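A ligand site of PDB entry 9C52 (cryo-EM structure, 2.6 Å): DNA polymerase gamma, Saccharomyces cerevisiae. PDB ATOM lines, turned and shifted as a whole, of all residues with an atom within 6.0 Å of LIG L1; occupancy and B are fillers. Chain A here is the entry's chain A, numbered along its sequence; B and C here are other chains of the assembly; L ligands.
O3' of DG 23 of chain B is covalently linked to a phosphorus (P1) of LIG L1, at 1.6 Å.
An oxygen (O4) of LIG L1 is in hydrogen-bond range of the guanidinium group (NH2) of Arg 629, at 3.2 Å.
The side-chain amino group of Lys 921 lies within salt-bridge range of an oxygen (O1) of LIG L1, 3.2 Å away.
N2 of LIG L1 sits at hydrogen-bond distance from N1 of DA 19 of chain C (3.4 Å).
N3 of LG2 L2 is in hydrogen-bond range of N6 of DA 19 of chain C (3.4 Å).
N3 of LG2 L2 sits at hydrogen-bond distance from O4 of DT 18 of chain C (2.6 Å).
The guanidinium group (NH2) of Arg 629 lies within hydrogen-bond range of a ring nitrogen (ND1) of His 864, at 3.3 Å.
CB of His 864 touches C6 of LIG L1, at 3.7 Å.
Within 4 Å of LIG L1: Arg 629, His 864, Lys 921, DG 23 of chain B and DA 19 of chain C.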
ATOM      1  N   ARG A 629      27.861  35.591 -18.939  1.00  0.00           N
ATOM      2  CA  ARG A 629      26.456  35.207 -18.904  1.00  0.00           C
ATOM      3  C   ARG A 629      25.704  36.042 -17.869  1.00  0.00           C
ATOM      4  O   ARG A 629      26.282  36.780 -17.075  1.00  0.00           O
ATOM      5  CB  ARG A 629      26.320  33.715 -18.614  1.00  0.00           C
ATOM      6  CG  ARG A 629      27.113  32.823 -19.548  1.00  0.00           C
ATOM      7  CD  ARG A 629      27.142  31.395 -19.045  1.00  0.00           C
ATOM      8  NE  ARG A 629      25.963  30.651 -19.471  1.00  0.00           N
ATOM      9  CZ  ARG A 629      25.767  29.353 -19.243  1.00  0.00           C
ATOM     10  NH1 ARG A 629      26.651  28.634 -18.569  1.00  0.00           N
ATOM     11  NH2 ARG A 629      24.663  28.783 -19.704  1.00  0.00           N
ATOM     12  N   LEU A 636      16.237  31.862 -12.841  1.00  0.00           N
ATOM     13  CA  LEU A 636      17.114  30.994 -13.613  1.00  0.00           C
ATOM     14  C   LEU A 636      17.502  29.738 -12.846  1.00  0.00           C
ATOM     15  O   LEU A 636      18.347  28.971 -13.317  1.00  0.00           O
ATOM     16  CB  LEU A 636      18.362  31.735 -14.076  1.00  0.00           C
ATOM     17  CG  LEU A 636      18.174  32.868 -15.088  1.00  0.00           C
ATOM     18  CD1 LEU A 636      19.481  33.582 -15.352  1.00  0.00           C
ATOM     19  CD2 LEU A 636      17.580  32.337 -16.373  1.00  0.00           C
ATOM     20  N   ALA A 638      14.741  27.963 -11.229  1.00  0.00           N
ATOM     21  CA  ALA A 638      13.447  27.355 -10.932  1.00  0.00           C
ATOM     22  C   ALA A 638      13.403  25.906 -11.416  1.00  0.00           C
ATOM     23  O   ALA A 638      13.906  25.574 -12.497  1.00  0.00           O
ATOM     24  CB  ALA A 638      12.330  28.155 -11.594  1.00  0.00           C
ATOM     25  N   ASN A 640      11.655  22.235 -12.588  1.00  0.00           N
ATOM     26  CA  ASN A 640      10.598  21.788 -13.485  1.00  0.00           C
ATOM     27  C   ASN A 640       9.575  20.947 -12.735  1.00  0.00           C
ATOM     28  O   ASN A 640       9.802  20.511 -11.605  1.00  0.00           O
ATOM     29  CB  ASN A 640      11.198  20.997 -14.656  1.00  0.00           C
ATOM     30  CG  ASN A 640      11.874  21.895 -15.673  1.00  0.00           C
ATOM     31  OD1 ASN A 640      11.250  22.745 -16.295  1.00  0.00           O
ATOM     32  ND2 ASN A 640      13.186  21.699 -15.845  1.00  0.00           N
ATOM     33  N   LYS A 651       6.923  28.026 -12.516  1.00  0.00           N
ATOM     34  CA  LYS A 651       6.932  28.694 -13.822  1.00  0.00           C
ATOM     35  C   LYS A 651       5.582  28.658 -14.513  1.00  0.00           C
ATOM     36  O   LYS A 651       5.383  29.412 -15.478  1.00  0.00           O
ATOM     37  CB  LYS A 651       8.002  28.091 -14.726  1.00  0.00           C
ATOM     38  CG  LYS A 651       9.423  28.321 -14.237  1.00  0.00           C
ATOM     39  CD  LYS A 651      10.434  27.939 -15.302  1.00  0.00           C
ATOM     40  CE  LYS A 651      10.512  26.438 -15.485  1.00  0.00           C
ATOM     41  NZ  LYS A 651      11.245  26.069 -16.723  1.00  0.00           N
ATOM     42  N   ILE A 863      16.074  32.856 -20.742  1.00  0.00           N
ATOM     43  CA  ILE A 863      16.904  31.905 -20.017  1.00  0.00           C
ATOM     44  C   ILE A 863      18.078  31.598 -20.941  1.00  0.00           C
ATOM     45  O   ILE A 863      18.056  31.998 -22.105  1.00  0.00           O
ATOM     46  CB  ILE A 863      16.067  30.663 -19.630  1.00  0.00           C
ATOM     47  CG1 ILE A 863      14.918  31.075 -18.708  1.00  0.00           C
ATOM     48  CG2 ILE A 863      16.873  29.629 -18.849  1.00  0.00           C
ATOM     49  CD1 ILE A 863      13.897  29.993 -18.479  1.00  0.00           C
ATOM     50  N   HIS A 864      19.120  30.949 -20.435  1.00  0.00           N
ATOM     51  CA  HIS A 864      20.236  30.533 -21.276  1.00  0.00           C
ATOM     52  C   HIS A 864      19.705  29.715 -22.451  1.00  0.00           C
ATOM     53  O   HIS A 864      18.794  28.910 -22.272  1.00  0.00           O
ATOM     54  CB  HIS A 864      21.245  29.728 -20.470  1.00  0.00           C
ATOM     55  CG  HIS A 864      21.820  30.457 -19.295  1.00  0.00           C
ATOM     56  ND1 HIS A 864      22.754  31.455 -19.417  1.00  0.00           N
ATOM     57  CD2 HIS A 864      21.582  30.321 -17.959  1.00  0.00           C
ATOM     58  CE1 HIS A 864      23.076  31.915 -18.223  1.00  0.00           C
ATOM     59  NE2 HIS A 864      22.373  31.240 -17.326  1.00  0.00           N
ATOM     60  N   ASP A 865      20.162  30.061 -23.663  1.00  0.00           N
ATOM     61  CA  ASP A 865      19.906  29.514 -25.013  1.00  0.00           C
ATOM     62  C   ASP A 865      18.416  29.259 -25.262  1.00  0.00           C
ATOM     63  O   ASP A 865      18.084  28.466 -26.137  1.00  0.00           O
ATOM     64  CB  ASP A 865      20.728  28.260 -25.393  1.00  0.00           C
ATOM     65  CG  ASP A 865      20.434  26.999 -24.564  1.00  0.00           C
ATOM     66  OD1 ASP A 865      19.614  26.984 -23.643  1.00  0.00           O
ATOM     67  OD2 ASP A 865      21.065  25.969 -24.876  1.00  0.00           O
ATOM     68  N   GLU A 866      17.522  29.915 -24.525  1.00  0.00           N
ATOM     69  CA  GLU A 866      16.080  29.783 -24.673  1.00  0.00           C
ATOM     70  C   GLU A 866      15.432  31.156 -24.551  1.00  0.00           C
ATOM     71  O   GLU A 866      15.726  31.905 -23.614  1.00  0.00           O
ATOM     72  CB  GLU A 866      15.518  28.833 -23.607  1.00  0.00           C
ATOM     73  CG  GLU A 866      14.051  28.481 -23.758  1.00  0.00           C
ATOM     74  CD  GLU A 866      13.467  27.957 -22.473  1.00  0.00           C
ATOM     75  OE1 GLU A 866      12.225  27.964 -22.315  1.00  0.00           O
ATOM     76  OE2 GLU A 866      14.261  27.529 -21.595  1.00  0.00           O
ATOM     77  N   LYS A 921       8.304  23.382 -19.993  1.00  0.00           N
ATOM     78  CA  LYS A 921       9.315  22.760 -20.853  1.00  0.00           C
ATOM     79  C   LYS A 921       8.695  22.158 -22.109  1.00  0.00           C
ATOM     80  O   LYS A 921       9.229  22.318 -23.214  1.00  0.00           O
ATOM     81  CB  LYS A 921      10.079  21.696 -20.068  1.00  0.00           C
ATOM     82  CG  LYS A 921      10.992  20.823 -20.923  1.00  0.00           C
ATOM     83  CD  LYS A 921      12.389  21.402 -21.005  1.00  0.00           C
ATOM     84  CE  LYS A 921      13.008  21.569 -19.628  1.00  0.00           C
ATOM     85  NZ  LYS A 921      14.371  22.154 -19.702  1.00  0.00           N
ATOM     86  P    DG B  23      16.508  21.013 -11.848  1.00  0.00           P
ATOM     87  OP1  DG B  23      15.189  20.833 -12.484  1.00  0.00           O
ATOM     88  OP2  DG B  23      17.494  19.906 -11.870  1.00  0.00           O
ATOM     89  O5'  DG B  23      17.191  22.311 -12.497  1.00  0.00           O
ATOM     90  C5'  DG B  23      16.465  23.528 -12.574  1.00  0.00           C
ATOM     91  C4'  DG B  23      17.306  24.628 -13.199  1.00  0.00           C
ATOM     92  O4'  DG B  23      18.393  24.965 -12.319  1.00  0.00           O
ATOM     93  C3'  DG B  23      17.980  24.248 -14.510  1.00  0.00           C
ATOM     94  O3'  DG B  23      17.070  24.449 -15.590  1.00  0.00           O
ATOM     95  C2'  DG B  23      19.130  25.233 -14.559  1.00  0.00           C
ATOM     96  C1'  DG B  23      19.514  25.370 -13.084  1.00  0.00           C
ATOM     97  N9   DG B  23      20.671  24.559 -12.708  1.00  0.00           N
ATOM     98  C8   DG B  23      20.645  23.360 -12.044  1.00  0.00           C
ATOM     99  N7   DG B  23      21.828  22.861 -11.833  1.00  0.00           N
ATOM    100  C5   DG B  23      22.701  23.785 -12.384  1.00  0.00           C
ATOM    101  C6   DG B  23      24.108  23.790 -12.461  1.00  0.00           C
ATOM    102  O6   DG B  23      24.893  22.943 -12.036  1.00  0.00           O
ATOM    103  N1   DG B  23      24.593  24.929 -13.106  1.00  0.00           N
ATOM    104  C2   DG B  23      23.805  25.929 -13.607  1.00  0.00           C
ATOM    105  N2   DG B  23      24.451  26.949 -14.195  1.00  0.00           N
ATOM    106  N3   DG B  23      22.478  25.938 -13.547  1.00  0.00           N
ATOM    107  C4   DG B  23      21.997  24.847 -12.926  1.00  0.00           C
ATOM    108  P    DT C  18      38.264  15.286 -13.147  1.00  0.00           P
ATOM    109  OP1  DT C  18      37.465  15.259 -11.893  1.00  0.00           O
ATOM    110  OP2  DT C  18      38.551  14.022 -13.851  1.00  0.00           O
ATOM    111  O5'  DT C  18      37.558  16.290 -14.175  1.00  0.00           O
ATOM    112  C5'  DT C  18      36.609  17.252 -13.704  1.00  0.00           C
ATOM    113  C4'  DT C  18      36.162  18.165 -14.829  1.00  0.00           C
ATOM    114  O4'  DT C  18      35.036  17.578 -15.514  1.00  0.00           O
ATOM    115  C3'  DT C  18      35.652  19.527 -14.404  1.00  0.00           C
ATOM    116  O3'  DT C  18      36.750  20.413 -14.190  1.00  0.00           O
ATOM    117  C2'  DT C  18      34.822  19.951 -15.618  1.00  0.00           C
ATOM    118  C1'  DT C  18      34.326  18.605 -16.180  1.00  0.00           C
ATOM    119  N1   DT C  18      32.857  18.390 -16.008  1.00  0.00           N
ATOM    120  C2   DT C  18      31.983  19.004 -16.872  1.00  0.00           C
ATOM    121  O2   DT C  18      32.342  19.718 -17.780  1.00  0.00           O
ATOM    122  N3   DT C  18      30.655  18.749 -16.628  1.00  0.00           N
ATOM    123  C4   DT C  18      30.133  17.954 -15.633  1.00  0.00           C
ATOM    124  O4   DT C  18      28.925  17.782 -15.491  1.00  0.00           O
ATOM    125  C5   DT C  18      31.101  17.342 -14.749  1.00  0.00           C
ATOM    126  C7   DT C  18      30.641  16.462 -13.624  1.00  0.00           C
ATOM    127  C6   DT C  18      32.399  17.592 -14.980  1.00  0.00           C
ATOM    128  P    DA C  19      36.574  21.682 -13.215  1.00  0.00           P
ATOM    129  OP1  DA C  19      37.921  22.237 -12.971  1.00  0.00           O
ATOM    130  OP2  DA C  19      35.739  21.265 -12.080  1.00  0.00           O
ATOM    131  O5'  DA C  19      35.733  22.727 -14.096  1.00  0.00           O
ATOM    132  C5'  DA C  19      36.351  23.411 -15.174  1.00  0.00           C
ATOM    133  C4'  DA C  19      35.333  24.209 -15.972  1.00  0.00           C
ATOM    134  O4'  DA C  19      34.329  23.315 -16.509  1.00  0.00           O
ATOM    135  C3'  DA C  19      34.540  25.224 -15.171  1.00  0.00           C
ATOM    136  O3'  DA C  19      35.261  26.443 -15.069  1.00  0.00           O
ATOM    137  C2'  DA C  19      33.273  25.402 -16.023  1.00  0.00           C
ATOM    138  C1'  DA C  19      33.121  24.025 -16.691  1.00  0.00           C
ATOM    139  N9   DA C  19      32.019  23.232 -16.150  1.00  0.00           N
ATOM    140  C8   DA C  19      32.114  22.024 -15.518  1.00  0.00           C
ATOM    141  N7   DA C  19      30.966  21.536 -15.137  1.00  0.00           N
ATOM    142  C5   DA C  19      30.045  22.486 -15.542  1.00  0.00           C
ATOM    143  C6   DA C  19      28.650  22.563 -15.432  1.00  0.00           C
ATOM    144  N6   DA C  19      27.902  21.620 -14.841  1.00  0.00           N
ATOM    145  N1   DA C  19      28.033  23.650 -15.931  1.00  0.00           N
ATOM    146  C2   DA C  19      28.779  24.602 -16.518  1.00  0.00           C
ATOM    147  N3   DA C  19      30.100  24.639 -16.679  1.00  0.00           N
ATOM    148  C4   DA C  19      30.678  23.543 -16.167  1.00  0.00           C
ATOM    149  P    DC C  20      35.079  27.398 -13.789  1.00  0.00           P
ATOM    150  OP1  DC C  20      36.123  28.443 -13.873  1.00  0.00           O
ATOM    151  OP2  DC C  20      34.998  26.526 -12.604  1.00  0.00           O
ATOM    152  O5'  DC C  20      33.640  28.070 -13.998  1.00  0.00           O
ATOM    153  C5'  DC C  20      33.489  29.209 -14.849  1.00  0.00           C
ATOM    154  C4'  DC C  20      32.027  29.565 -15.004  1.00  0.00           C
ATOM    155  O4'  DC C  20      31.286  28.381 -15.341  1.00  0.00           O
ATOM    156  C3'  DC C  20      31.359  30.106 -13.756  1.00  0.00           C
ATOM    157  O3'  DC C  20      31.528  31.522 -13.689  1.00  0.00           O
ATOM    158  C2'  DC C  20      29.890  29.733 -13.960  1.00  0.00           C
ATOM    159  C1'  DC C  20      29.955  28.501 -14.881  1.00  0.00           C
ATOM    160  N1   DC C  20      29.573  27.225 -14.211  1.00  0.00           N
ATOM    161  C2   DC C  20      28.228  26.959 -13.936  1.00  0.00           C
ATOM    162  O2   DC C  20      27.368  27.799 -14.234  1.00  0.00           O
ATOM    163  N3   DC C  20      27.895  25.784 -13.340  1.00  0.00           N
ATOM    164  C4   DC C  20      28.844  24.906 -13.039  1.00  0.00           C
ATOM    165  N4   DC C  20      28.479  23.761 -12.458  1.00  0.00           N
ATOM    166  C5   DC C  20      30.229  25.152 -13.317  1.00  0.00           C
ATOM    167  C6   DC C  20      30.534  26.314 -13.904  1.00  0.00           C
HETATM  168  P1  LIG L   1      17.588  23.741 -16.878  1.00  0.00           P
HETATM  169  O1  LIG L   1      16.288  23.773 -17.645  1.00  0.00           O
HETATM  170  O2  LIG L   1      17.940  22.311 -16.554  1.00  0.00           O
HETATM  171  O3  LIG L   1      18.787  24.402 -17.796  1.00  0.00           O
HETATM  172  N1  LIG L   1      22.499  25.159 -17.384  1.00  0.00           N
HETATM  173  C1  LIG L   1      21.806  24.036 -16.791  1.00  0.00           C
HETATM  174  C2  LIG L   1      23.984  25.155 -17.454  1.00  0.00           C
HETATM  175  O4  LIG L   1      24.559  26.072 -17.933  1.00  0.00           O
HETATM  176  N2  LIG L   1      24.763  24.001 -16.908  1.00  0.00           N
HETATM  177  C3  LIG L   1      24.061  22.875 -16.314  1.00  0.00           C
HETATM  178  O5  LIG L   1      24.670  21.959 -15.883  1.00  0.00           O
HETATM  179  C4  LIG L   1      22.576  22.879 -16.244  1.00  0.00           C
HETATM  180  C5  LIG L   1      21.829  21.700 -15.623  1.00  0.00           C
HETATM  181  C6  LIG L   1      21.686  26.214 -19.527  1.00  0.00           C
HETATM  182  C7  LIG L   1      18.477  25.534 -18.561  1.00  0.00           C
HETATM  183  C8  LIG L   1      19.612  26.338 -18.707  1.00  0.00           C
HETATM  184  O6  LIG L   1      20.540  26.251 -17.461  1.00  0.00           O
HETATM  185  C9  LIG L   1      21.743  26.275 -17.907  1.00  0.00           C
HETATM  186  C10 LIG L   1      20.483  25.847 -19.853  1.00  0.00           C
HETATM  187  P1  LG2 L   2      19.373  20.144 -26.475  1.00  0.00           P
HETATM  188  O1  LG2 L   2      18.427  19.102 -25.954  1.00  0.00           O
HETATM  189  O2  LG2 L   2      18.773  21.526 -26.259  1.00  0.00           O
HETATM  190  O3  LG2 L   2      19.606  19.925 -27.952  1.00  0.00           O
HETATM  191  P2  LG2 L   2      21.928  21.268 -25.566  1.00  0.00           P
HETATM  192  O4  LG2 L   2      21.464  22.471 -26.356  1.00  0.00           O
HETATM  193  O5  LG2 L   2      23.286  20.792 -26.117  1.00  0.00           O
HETATM  194  O6  LG2 L   2      20.806  20.039 -25.671  1.00  0.00           O
HETATM  195  P3  LG2 L   2      21.119  22.803 -23.158  1.00  0.00           P
HETATM  196  O7  LG2 L   2      20.011  23.272 -24.073  1.00  0.00           O
HETATM  197  O8  LG2 L   2      20.508  22.149 -21.915  1.00  0.00           O
HETATM  198  O9  LG2 L   2      22.103  21.702 -23.946  1.00  0.00           O
HETATM  199  O10 LG2 L   2      22.056  24.113 -22.708  1.00  0.00           O
HETATM  200  C1  LG2 L   2      23.112  23.871 -21.842  1.00  0.00           C
HETATM  201  C2  LG2 L   2      24.382  24.552 -22.334  1.00  0.00           C
HETATM  202  O11 LG2 L   2      25.496  24.545 -21.157  1.00  0.00           O
HETATM  203  C3  LG2 L   2      24.892  23.882 -23.341  1.00  0.00           C
HETATM  204  O12 LG2 L   2      25.437  24.846 -24.355  1.00  0.00           O
HETATM  205  C4  LG2 L   2      26.038  23.035 -22.781  1.00  0.00           C
HETATM  206  C5  LG2 L   2      26.265  23.510 -21.326  1.00  0.00           C
HETATM  207  N1  LG2 L   2      25.916  22.421 -20.339  1.00  0.00           N
HETATM  208  C6  LG2 L   2      24.829  21.792 -19.861  1.00  0.00           C
HETATM  209  N2  LG2 L   2      25.255  20.889 -18.992  1.00  0.00           N
HETATM  210  C7  LG2 L   2      26.589  20.968 -18.939  1.00  0.00           C
HETATM  211  C8  LG2 L   2      27.526  20.248 -18.196  1.00  0.00           C
HETATM  212  N3  LG2 L   2      27.484  19.131 -17.155  1.00  0.00           N
HETATM  213  N4  LG2 L   2      28.803  20.518 -18.317  1.00  0.00           N
HETATM  214  C9  LG2 L   2      29.224  21.495 -19.186  1.00  0.00           C
HETATM  215  N5  LG2 L   2      28.317  22.194 -19.910  1.00  0.00           N
HETATM  216  C10 LG2 L   2      27.000  21.914 -19.777  1.00  0.00           C
